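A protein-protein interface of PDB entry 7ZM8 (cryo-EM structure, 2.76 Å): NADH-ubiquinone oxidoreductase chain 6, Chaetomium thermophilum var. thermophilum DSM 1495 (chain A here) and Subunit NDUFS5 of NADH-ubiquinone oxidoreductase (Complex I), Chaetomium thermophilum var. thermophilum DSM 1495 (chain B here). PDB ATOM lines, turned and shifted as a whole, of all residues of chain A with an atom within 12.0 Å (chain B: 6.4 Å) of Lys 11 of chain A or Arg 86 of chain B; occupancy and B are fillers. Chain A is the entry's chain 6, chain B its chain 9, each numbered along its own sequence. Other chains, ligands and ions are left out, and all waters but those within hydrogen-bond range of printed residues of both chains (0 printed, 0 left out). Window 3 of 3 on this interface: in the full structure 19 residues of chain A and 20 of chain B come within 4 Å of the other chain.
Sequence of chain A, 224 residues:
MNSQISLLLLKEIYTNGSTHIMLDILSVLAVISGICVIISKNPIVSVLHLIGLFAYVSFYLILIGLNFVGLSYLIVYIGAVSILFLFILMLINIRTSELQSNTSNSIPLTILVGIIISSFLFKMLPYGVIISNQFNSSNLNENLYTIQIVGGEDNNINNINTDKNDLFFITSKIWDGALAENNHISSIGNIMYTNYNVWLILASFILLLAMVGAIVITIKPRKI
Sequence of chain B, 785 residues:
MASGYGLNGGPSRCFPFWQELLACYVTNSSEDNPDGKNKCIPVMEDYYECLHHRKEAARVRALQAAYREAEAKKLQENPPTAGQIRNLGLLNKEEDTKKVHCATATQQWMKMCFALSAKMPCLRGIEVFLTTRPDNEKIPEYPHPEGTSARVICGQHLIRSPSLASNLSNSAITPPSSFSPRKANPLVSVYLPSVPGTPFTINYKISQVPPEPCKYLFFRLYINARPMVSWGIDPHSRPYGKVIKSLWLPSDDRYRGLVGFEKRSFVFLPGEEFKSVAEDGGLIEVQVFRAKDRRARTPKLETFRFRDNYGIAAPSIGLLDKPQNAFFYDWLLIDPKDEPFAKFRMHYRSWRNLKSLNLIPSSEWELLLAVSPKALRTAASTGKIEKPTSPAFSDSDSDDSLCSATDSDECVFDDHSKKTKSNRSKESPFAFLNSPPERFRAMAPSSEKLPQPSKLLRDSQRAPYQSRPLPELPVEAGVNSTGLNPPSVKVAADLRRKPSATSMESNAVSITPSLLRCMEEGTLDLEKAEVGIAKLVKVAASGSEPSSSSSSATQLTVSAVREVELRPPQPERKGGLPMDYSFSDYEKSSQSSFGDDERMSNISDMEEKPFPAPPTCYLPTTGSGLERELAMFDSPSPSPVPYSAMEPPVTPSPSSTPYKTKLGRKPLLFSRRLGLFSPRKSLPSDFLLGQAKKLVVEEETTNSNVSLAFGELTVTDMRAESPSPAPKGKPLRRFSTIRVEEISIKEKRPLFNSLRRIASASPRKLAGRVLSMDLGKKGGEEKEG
CD1 of Leu 8 of chain A touches CG2 of Ile 85 of chain B, 3.8 Å away.
CG1 of Val 100 of chain B touches CD1 of Leu 8 of chain A, at 3.9 Å.
Leu 10 of chain A touches Ala 82 of chain B.
CD2 of Leu 10 of chain A touches O of Ile 85 of chain B (3.4 Å).
The backbone carbonyl oxygen (O) of Lys 11 of chain A is in hydrogen-bond range of the guanidinium group (NH1) of Arg 86 of chain B (2.7 Å).
Printed residues of chain B within 4 Å of Leu 8 of chain A: Ile 85 (3.8 Å) and Val 100 (3.9 Å).
Printed residues of chain B within 4 Å of Leu 10 of chain A: Ala 82 and Ile 85.
Of the printed residues of chain B, Lys 11 of chain A touches Arg 86 (2.7 Å).
Printed residues of chain A within 4 Å of Ala 82 of chain B: Leu 10 (3.6 Å).
No residue of chain A comes within 4 Å of Gly 83 of chain B.
Of chain A, only Lys 11 (2.7 Å) comes within 4 Å of Arg 86 of chain B.
No residue of chain A comes within 4 Å of Asn 87 of chain B.
No residue of chain A comes within 4 Å of Leu 88 of chain B.
Printed residues of chain A within 4 Å of Val 100 of chain B: Leu 8 (3.9 Å).
The nearest residue of chain B that does not touch Lys 11 of chain A is Ala 82 of chain B (5.5 Å).
The nearest printed residue of chain B that does not touch Leu 10 of chain A is Arg 86 of chain B (4.4 Å).
Of the 10 printed residues of chain B, 4 touch a printed residue of chain A.
Printed residues of chain B that touch a printed residue of chain A: Ala 82, Ile 85, Arg 86 and Val 100.
Hydrophobic or aromatic side chains of chain B that line the printed part of chain A: Ile 85 and Val 100.
Of the 16 printed residues of chain A, 3 touch a printed residue of chain B.
Along chain A the printed residues that touch a printed residue of chain B span positions 8 to 11.
Among the printed residues, no Asp or Glu carboxylate lies within 4 Å of a Lys or Arg side-chain nitrogen of the other chain.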
ATOM      1  N   LEU A   7     -24.733  24.473  -4.248  1.00  0.00           N
ATOM      2  CA  LEU A   7     -25.132  23.921  -5.562  1.00  0.00           C
ATOM      3  C   LEU A   7     -24.081  22.901  -5.983  1.00  0.00           C
ATOM      4  O   LEU A   7     -22.904  23.254  -5.988  1.00  0.00           O
ATOM      5  CB  LEU A   7     -25.262  25.048  -6.590  1.00  0.00           C
ATOM      6  CG  LEU A   7     -26.315  26.112  -6.307  1.00  0.00           C
ATOM      7  CD1 LEU A   7     -26.203  27.233  -7.327  1.00  0.00           C
ATOM      8  CD2 LEU A   7     -27.711  25.512  -6.323  1.00  0.00           C
ATOM      9  N   LEU A   8     -24.509  21.676  -6.303  1.00  0.00           N
ATOM     10  CA  LEU A   8     -23.575  20.590  -6.701  1.00  0.00           C
ATOM     11  C   LEU A   8     -23.983  20.028  -8.067  1.00  0.00           C
ATOM     12  O   LEU A   8     -25.161  19.692  -8.228  1.00  0.00           O
ATOM     13  CB  LEU A   8     -23.625  19.497  -5.632  1.00  0.00           C
ATOM     14  CG  LEU A   8     -23.137  19.897  -4.242  1.00  0.00           C
ATOM     15  CD1 LEU A   8     -23.533  18.847  -3.219  1.00  0.00           C
ATOM     16  CD2 LEU A   8     -21.633  20.097  -4.239  1.00  0.00           C
ATOM     17  N   LEU A   9     -23.026  19.873  -8.988  1.00  0.00           N
ATOM     18  CA  LEU A   9     -23.317  19.359 -10.355  1.00  0.00           C
ATOM     19  C   LEU A   9     -22.732  17.949 -10.510  1.00  0.00           C
ATOM     20  O   LEU A   9     -21.542  17.786 -10.222  1.00  0.00           O
ATOM     21  CB  LEU A   9     -22.732  20.337 -11.377  1.00  0.00           C
ATOM     22  CG  LEU A   9     -23.391  20.331 -12.754  1.00  0.00           C
ATOM     23  CD1 LEU A   9     -24.894  20.532 -12.636  1.00  0.00           C
ATOM     24  CD2 LEU A   9     -22.781  21.403 -13.639  1.00  0.00           C
ATOM     25  N   LEU A  10     -23.543  16.973 -10.930  1.00  0.00           N
ATOM     26  CA  LEU A  10     -23.095  15.557 -11.048  1.00  0.00           C
ATOM     27  C   LEU A  10     -23.531  14.994 -12.403  1.00  0.00           C
ATOM     28  O   LEU A  10     -24.484  15.532 -12.971  1.00  0.00           O
ATOM     29  CB  LEU A  10     -23.771  14.729  -9.952  1.00  0.00           C
ATOM     30  CG  LEU A  10     -23.198  14.830  -8.546  1.00  0.00           C
ATOM     31  CD1 LEU A  10     -24.035  15.777  -7.700  1.00  0.00           C
ATOM     32  CD2 LEU A  10     -23.168  13.448  -7.916  1.00  0.00           C
ATOM     33  N   LYS A  11     -22.869  13.944 -12.889  1.00  0.00           N
ATOM     34  CA  LYS A  11     -23.301  13.285 -14.150  1.00  0.00           C
ATOM     35  C   LYS A  11     -24.319  12.188 -13.832  1.00  0.00           C
ATOM     36  O   LYS A  11     -24.029  11.372 -12.950  1.00  0.00           O
ATOM     37  CB  LYS A  11     -22.113  12.678 -14.895  1.00  0.00           C
ATOM     38  CG  LYS A  11     -22.402  12.233 -16.321  1.00  0.00           C
ATOM     39  CD  LYS A  11     -21.174  11.754 -17.063  1.00  0.00           C
ATOM     40  CE  LYS A  11     -21.456  11.409 -18.510  1.00  0.00           C
ATOM     41  NZ  LYS A  11     -20.226  10.997 -19.226  1.00  0.00           N
ATOM     42  N   GLU A  12     -25.473  12.187 -14.513  1.00  0.00           N
ATOM     43  CA  GLU A  12     -26.473  11.101 -14.338  1.00  0.00           C
ATOM     44  C   GLU A  12     -25.902   9.776 -14.851  1.00  0.00           C
ATOM     45  O   GLU A  12     -25.082   9.815 -15.781  1.00  0.00           O
ATOM     46  CB  GLU A  12     -27.764  11.464 -15.063  1.00  0.00           C
ATOM     47  CG  GLU A  12     -28.167  12.907 -14.864  1.00  0.00           C
ATOM     48  CD  GLU A  12     -29.402  13.301 -15.647  1.00  0.00           C
ATOM     49  OE1 GLU A  12     -29.718  14.501 -15.690  1.00  0.00           O
ATOM     50  OE2 GLU A  12     -30.043  12.402 -16.204  1.00  0.00           O
ATOM     51  N   ILE A  13     -26.351   8.646 -14.302  1.00  0.00           N
ATOM     52  CA  ILE A  13     -25.723   7.361 -14.721  1.00  0.00           C
ATOM     53  C   ILE A  13     -26.648   6.463 -15.563  1.00  0.00           C
ATOM     54  O   ILE A  13     -26.173   5.995 -16.614  1.00  0.00           O
ATOM     55  CB  ILE A  13     -25.056   6.663 -13.515  1.00  0.00           C
ATOM     56  CG1 ILE A  13     -24.384   5.346 -13.909  1.00  0.00           C
ATOM     57  CG2 ILE A  13     -26.034   6.492 -12.363  1.00  0.00           C
ATOM     58  CD1 ILE A  13     -23.559   4.727 -12.806  1.00  0.00           C
ATOM     59  N   TYR A  14     -27.896   6.214 -15.163  1.00  0.00           N
ATOM     60  CA  TYR A  14     -28.716   5.250 -15.956  1.00  0.00           C
ATOM     61  C   TYR A  14     -29.933   5.925 -16.589  1.00  0.00           C
ATOM     62  O   TYR A  14     -30.611   5.280 -17.406  1.00  0.00           O
ATOM     63  CB  TYR A  14     -29.097   4.036 -15.114  1.00  0.00           C
ATOM     64  CG  TYR A  14     -27.932   3.175 -14.703  1.00  0.00           C
ATOM     65  CD1 TYR A  14     -27.286   2.362 -15.620  1.00  0.00           C
ATOM     66  CD2 TYR A  14     -27.473   3.165 -13.396  1.00  0.00           C
ATOM     67  CE1 TYR A  14     -26.216   1.566 -15.254  1.00  0.00           C
ATOM     68  CE2 TYR A  14     -26.403   2.374 -13.013  1.00  0.00           C
ATOM     69  CZ  TYR A  14     -25.772   1.571 -13.944  1.00  0.00           C
ATOM     70  OH  TYR A  14     -24.720   0.788 -13.570  1.00  0.00           O
ATOM     71  N   THR A  15     -30.186   7.185 -16.240  1.00  0.00           N
ATOM     72  CA  THR A  15     -31.325   7.957 -16.789  1.00  0.00           C
ATOM     73  C   THR A  15     -30.699   9.153 -17.499  1.00  0.00           C
ATOM     74  O   THR A  15     -31.280  10.237 -17.415  1.00  0.00           O
ATOM     75  CB  THR A  15     -32.241   8.355 -15.630  1.00  0.00           C
ATOM     76  OG1 THR A  15     -31.430   9.027 -14.666  1.00  0.00           O
ATOM     77  CG2 THR A  15     -32.910   7.166 -14.974  1.00  0.00           C
ATOM     78  N   ASN A  16     -29.605   8.946 -18.232  1.00  0.00           N
ATOM     79  CA  ASN A  16     -28.797  10.065 -18.784  1.00  0.00           C
ATOM     80  C   ASN A  16     -29.245  10.583 -20.152  1.00  0.00           C
ATOM     81  O   ASN A  16     -28.398  11.180 -20.812  1.00  0.00           O
ATOM     82  CB  ASN A  16     -27.312   9.709 -18.833  1.00  0.00           C
ATOM     83  CG  ASN A  16     -27.044   8.385 -19.518  1.00  0.00           C
ATOM     84  OD1 ASN A  16     -27.500   7.339 -19.062  1.00  0.00           O
ATOM     85  ND2 ASN A  16     -26.294   8.421 -20.606  1.00  0.00           N
ATOM     86  N   GLY A  17     -30.445  10.280 -20.632  1.00  0.00           N
ATOM     87  CA  GLY A  17     -30.935  10.913 -21.880  1.00  0.00           C
ATOM     88  C   GLY A  17     -30.014  10.805 -23.088  1.00  0.00           C
ATOM     89  O   GLY A  17     -29.325   9.777 -23.209  1.00  0.00           O
ATOM     90  N   SER A  18     -30.021  11.810 -23.972  1.00  0.00           N
ATOM     91  CA  SER A  18     -29.240  11.745 -25.232  1.00  0.00           C
ATOM     92  C   SER A  18     -28.306  12.944 -25.285  1.00  0.00           C
ATOM     93  O   SER A  18     -28.338  13.759 -24.367  1.00  0.00           O
ATOM     94  CB  SER A  18     -30.129  11.745 -26.432  1.00  0.00           C
ATOM     95  OG  SER A  18     -30.904  10.558 -26.485  1.00  0.00           O
ATOM     96  N   THR A  19     -27.524  13.064 -26.345  1.00  0.00           N
ATOM     97  CA  THR A  19     -26.532  14.161 -26.406  1.00  0.00           C
ATOM     98  C   THR A  19     -27.049  15.275 -27.314  1.00  0.00           C
ATOM     99  O   THR A  19     -27.716  14.964 -28.300  1.00  0.00           O
ATOM    100  CB  THR A  19     -25.126  13.643 -26.736  1.00  0.00           C
ATOM    101  OG1 THR A  19     -24.191  14.666 -26.398  1.00  0.00           O
ATOM    102  CG2 THR A  19     -24.952  13.234 -28.180  1.00  0.00           C
ATOM    103  N   HIS A  20     -26.791  16.521 -26.946  1.00  0.00           N
ATOM    104  CA  HIS A  20     -27.190  17.689 -27.763  1.00  0.00           C
ATOM    105  C   HIS A  20     -26.411  17.673 -29.076  1.00  0.00           C
ATOM    106  O   HIS A  20     -26.871  18.274 -30.048  1.00  0.00           O
ATOM    107  CB  HIS A  20     -26.938  18.971 -26.962  1.00  0.00           C
ATOM    108  CG  HIS A  20     -25.570  19.055 -26.376  1.00  0.00           C
ATOM    109  ND1 HIS A  20     -25.257  18.503 -25.150  1.00  0.00           N
ATOM    110  CD2 HIS A  20     -24.437  19.630 -26.833  1.00  0.00           C
ATOM    111  CE1 HIS A  20     -23.988  18.728 -24.881  1.00  0.00           C
ATOM    112  NE2 HIS A  20     -23.462  19.418 -25.898  1.00  0.00           N
ATOM    113  N   ILE A  21     -25.265  17.014 -29.095  1.00  0.00           N
ATOM    114  CA  ILE A  21     -24.398  17.027 -30.303  1.00  0.00           C
ATOM    115  C   ILE A  21     -25.170  16.449 -31.484  1.00  0.00           C
ATOM    116  O   ILE A  21     -25.046  17.008 -32.579  1.00  0.00           O
ATOM    117  CB  ILE A  21     -23.105  16.235 -30.025  1.00  0.00           C
ATOM    118  CG1 ILE A  21     -22.316  16.848 -28.865  1.00  0.00           C
ATOM    119  CG2 ILE A  21     -22.251  16.116 -31.277  1.00  0.00           C
ATOM    120  CD1 ILE A  21     -21.859  18.264 -29.125  1.00  0.00           C
ATOM    121  N   PHE A 168     -28.634  26.798 -18.462  1.00  0.00           N
ATOM    122  CA  PHE A 168     -28.976  25.361 -18.542  1.00  0.00           C
ATOM    123  C   PHE A 168     -30.475  25.283 -18.267  1.00  0.00           C
ATOM    124  O   PHE A 168     -30.963  26.105 -17.497  1.00  0.00           O
ATOM    125  CB  PHE A 168     -28.169  24.552 -17.525  1.00  0.00           C
ATOM    126  CG  PHE A 168     -26.800  24.115 -17.979  1.00  0.00           C
ATOM    127  CD1 PHE A 168     -25.712  24.966 -17.882  1.00  0.00           C
ATOM    128  CD2 PHE A 168     -26.596  22.843 -18.486  1.00  0.00           C
ATOM    129  CE1 PHE A 168     -24.453  24.559 -18.294  1.00  0.00           C
ATOM    130  CE2 PHE A 168     -25.337  22.436 -18.898  1.00  0.00           C
ATOM    131  CZ  PHE A 168     -24.268  23.295 -18.801  1.00  0.00           C
ATOM    132  N   THR B  81     -16.303  14.318  -4.135  1.00  0.00           N
ATOM    133  CA  THR B  81     -16.329  13.559  -5.373  1.00  0.00           C
ATOM    134  C   THR B  81     -17.761  13.172  -5.719  1.00  0.00           C
ATOM    135  O   THR B  81     -18.667  13.237  -4.885  1.00  0.00           O
ATOM    136  CB  THR B  81     -15.452  12.310  -5.262  1.00  0.00           C
ATOM    137  OG1 THR B  81     -15.404  11.645  -6.530  1.00  0.00           O
ATOM    138  CG2 THR B  81     -16.005  11.357  -4.220  1.00  0.00           C
ATOM    139  N   ALA B  82     -17.974  12.787  -6.978  1.00  0.00           N
ATOM    140  CA  ALA B  82     -19.355  12.465  -7.388  1.00  0.00           C
ATOM    141  C   ALA B  82     -19.815  11.221  -6.629  1.00  0.00           C
ATOM    142  O   ALA B  82     -20.983  11.194  -6.223  1.00  0.00           O
ATOM    143  CB  ALA B  82     -19.442  12.287  -8.882  1.00  0.00           C
ATOM    144  N   GLY B  83     -18.949  10.220  -6.481  1.00  0.00           N
ATOM    145  CA  GLY B  83     -19.366   9.025  -5.768  1.00  0.00           C
ATOM    146  C   GLY B  83     -19.810   9.322  -4.351  1.00  0.00           C
ATOM    147  O   GLY B  83     -20.702   8.661  -3.817  1.00  0.00           O
ATOM    148  N   GLN B  84     -19.177  10.308  -3.716  1.00  0.00           N
ATOM    149  CA  GLN B  84     -19.641  10.759  -2.410  1.00  0.00           C
ATOM    150  C   GLN B  84     -21.039  11.357  -2.501  1.00  0.00           C
ATOM    151  O   GLN B  84     -21.871  11.141  -1.614  1.00  0.00           O
ATOM    152  CB  GLN B  84     -18.657  11.769  -1.828  1.00  0.00           C
ATOM    153  CG  GLN B  84     -17.653  11.162  -0.873  1.00  0.00           C
ATOM    154  CD  GLN B  84     -16.440  12.043  -0.668  1.00  0.00           C
ATOM    155  OE1 GLN B  84     -16.312  13.098  -1.286  1.00  0.00           O
ATOM    156  NE2 GLN B  84     -15.538  11.612   0.207  1.00  0.00           N
ATOM    157  N   ILE B  85     -21.318  12.121  -3.569  1.00  0.00           N
ATOM    158  CA  ILE B  85     -22.641  12.809  -3.721  1.00  0.00           C
ATOM    159  C   ILE B  85     -23.610  11.875  -4.450  1.00  0.00           C
ATOM    160  O   ILE B  85     -24.585  12.379  -5.024  1.00  0.00           O
ATOM    161  CB  ILE B  85     -22.518  14.175  -4.434  1.00  0.00           C
ATOM    162  CG1 ILE B  85     -21.154  14.828  -4.217  1.00  0.00           C
ATOM    163  CG2 ILE B  85     -23.640  15.110  -4.007  1.00  0.00           C
ATOM    164  CD1 ILE B  85     -20.925  16.048  -5.072  1.00  0.00           C
ATOM    165  N   ARG B  86     -23.327  10.574  -4.471  1.00  0.00           N
ATOM    166  CA  ARG B  86     -24.258   9.577  -5.057  1.00  0.00           C
ATOM    167  C   ARG B  86     -24.619   8.683  -3.878  1.00  0.00           C
ATOM    168  O   ARG B  86     -25.557   7.877  -3.995  1.00  0.00           O
ATOM    169  CB  ARG B  86     -23.579   8.828  -6.205  1.00  0.00           C
ATOM    170  CG  ARG B  86     -24.428   8.727  -7.463  1.00  0.00           C
ATOM    171  CD  ARG B  86     -23.711   8.022  -8.597  1.00  0.00           C
ATOM    172  NE  ARG B  86     -22.639   8.807  -9.189  1.00  0.00           N
ATOM    173  CZ  ARG B  86     -22.804   9.651 -10.200  1.00  0.00           C
ATOM    174  NH1 ARG B  86     -24.005   9.827 -10.719  1.00  0.00           N
ATOM    175  NH2 ARG B  86     -21.773  10.319 -10.685  1.00  0.00           N
ATOM    176  N   ASN B  87     -23.865   8.831  -2.791  1.00  0.00           N
ATOM    177  CA  ASN B  87     -24.186   8.128  -1.565  1.00  0.00           C
ATOM    178  C   ASN B  87     -24.928   9.009  -0.576  1.00  0.00           C
ATOM    179  O   ASN B  87     -25.319   8.529   0.493  1.00  0.00           O
ATOM    180  CB  ASN B  87     -22.906   7.583  -0.933  1.00  0.00           C
ATOM    181  CG  ASN B  87     -22.308   6.457  -1.734  1.00  0.00           C
ATOM    182  OD1 ASN B  87     -23.021   5.585  -2.226  1.00  0.00           O
ATOM    183  ND2 ASN B  87     -20.991   6.471  -1.881  1.00  0.00           N
ATOM    184  N   LEU B  88     -25.039  10.303  -0.905  1.00  0.00           N
ATOM    185  CA  LEU B  88     -25.834  11.221  -0.048  1.00  0.00           C
ATOM    186  C   LEU B  88     -27.231  10.684   0.256  1.00  0.00           C
ATOM    187  O   LEU B  88     -27.905  10.244  -0.692  1.00  0.00           O
ATOM    188  CB  LEU B  88     -25.935  12.554  -0.795  1.00  0.00           C
ATOM    189  CG  LEU B  88     -26.946  13.559  -0.251  1.00  0.00           C
ATOM    190  CD1 LEU B  88     -26.541  14.027   1.136  1.00  0.00           C
ATOM    191  CD2 LEU B  88     -27.081  14.743  -1.191  1.00  0.00           C
ATOM    192  N   LEU B  90     -28.250   8.030   1.674  1.00  0.00           N
ATOM    193  CA  LEU B  90     -28.436   6.560   1.597  1.00  0.00           C
ATOM    194  C   LEU B  90     -28.396   6.002   3.013  1.00  0.00           C
ATOM    195  O   LEU B  90     -27.770   6.645   3.875  1.00  0.00           O
ATOM    196  CB  LEU B  90     -27.369   5.952   0.684  1.00  0.00           C
ATOM    197  CG  LEU B  90     -27.816   5.625  -0.741  1.00  0.00           C
ATOM    198  CD1 LEU B  90     -28.450   6.827  -1.421  1.00  0.00           C
ATOM    199  CD2 LEU B  90     -26.653   5.101  -1.565  1.00  0.00           C
ATOM    200  N   VAL B 100     -20.958  15.662   2.404  1.00  0.00           N
ATOM    201  CA  VAL B 100     -21.707  16.446   1.429  1.00  0.00           C
ATOM    202  C   VAL B 100     -22.342  17.652   2.102  1.00  0.00           C
ATOM    203  O   VAL B 100     -22.317  18.770   1.575  1.00  0.00           O
ATOM    204  CB  VAL B 100     -22.757  15.566   0.726  1.00  0.00           C
ATOM    205  CG1 VAL B 100     -23.690  16.414  -0.115  1.00  0.00           C
ATOM    206  CG2 VAL B 100     -22.080  14.522  -0.145  1.00  0.00           C
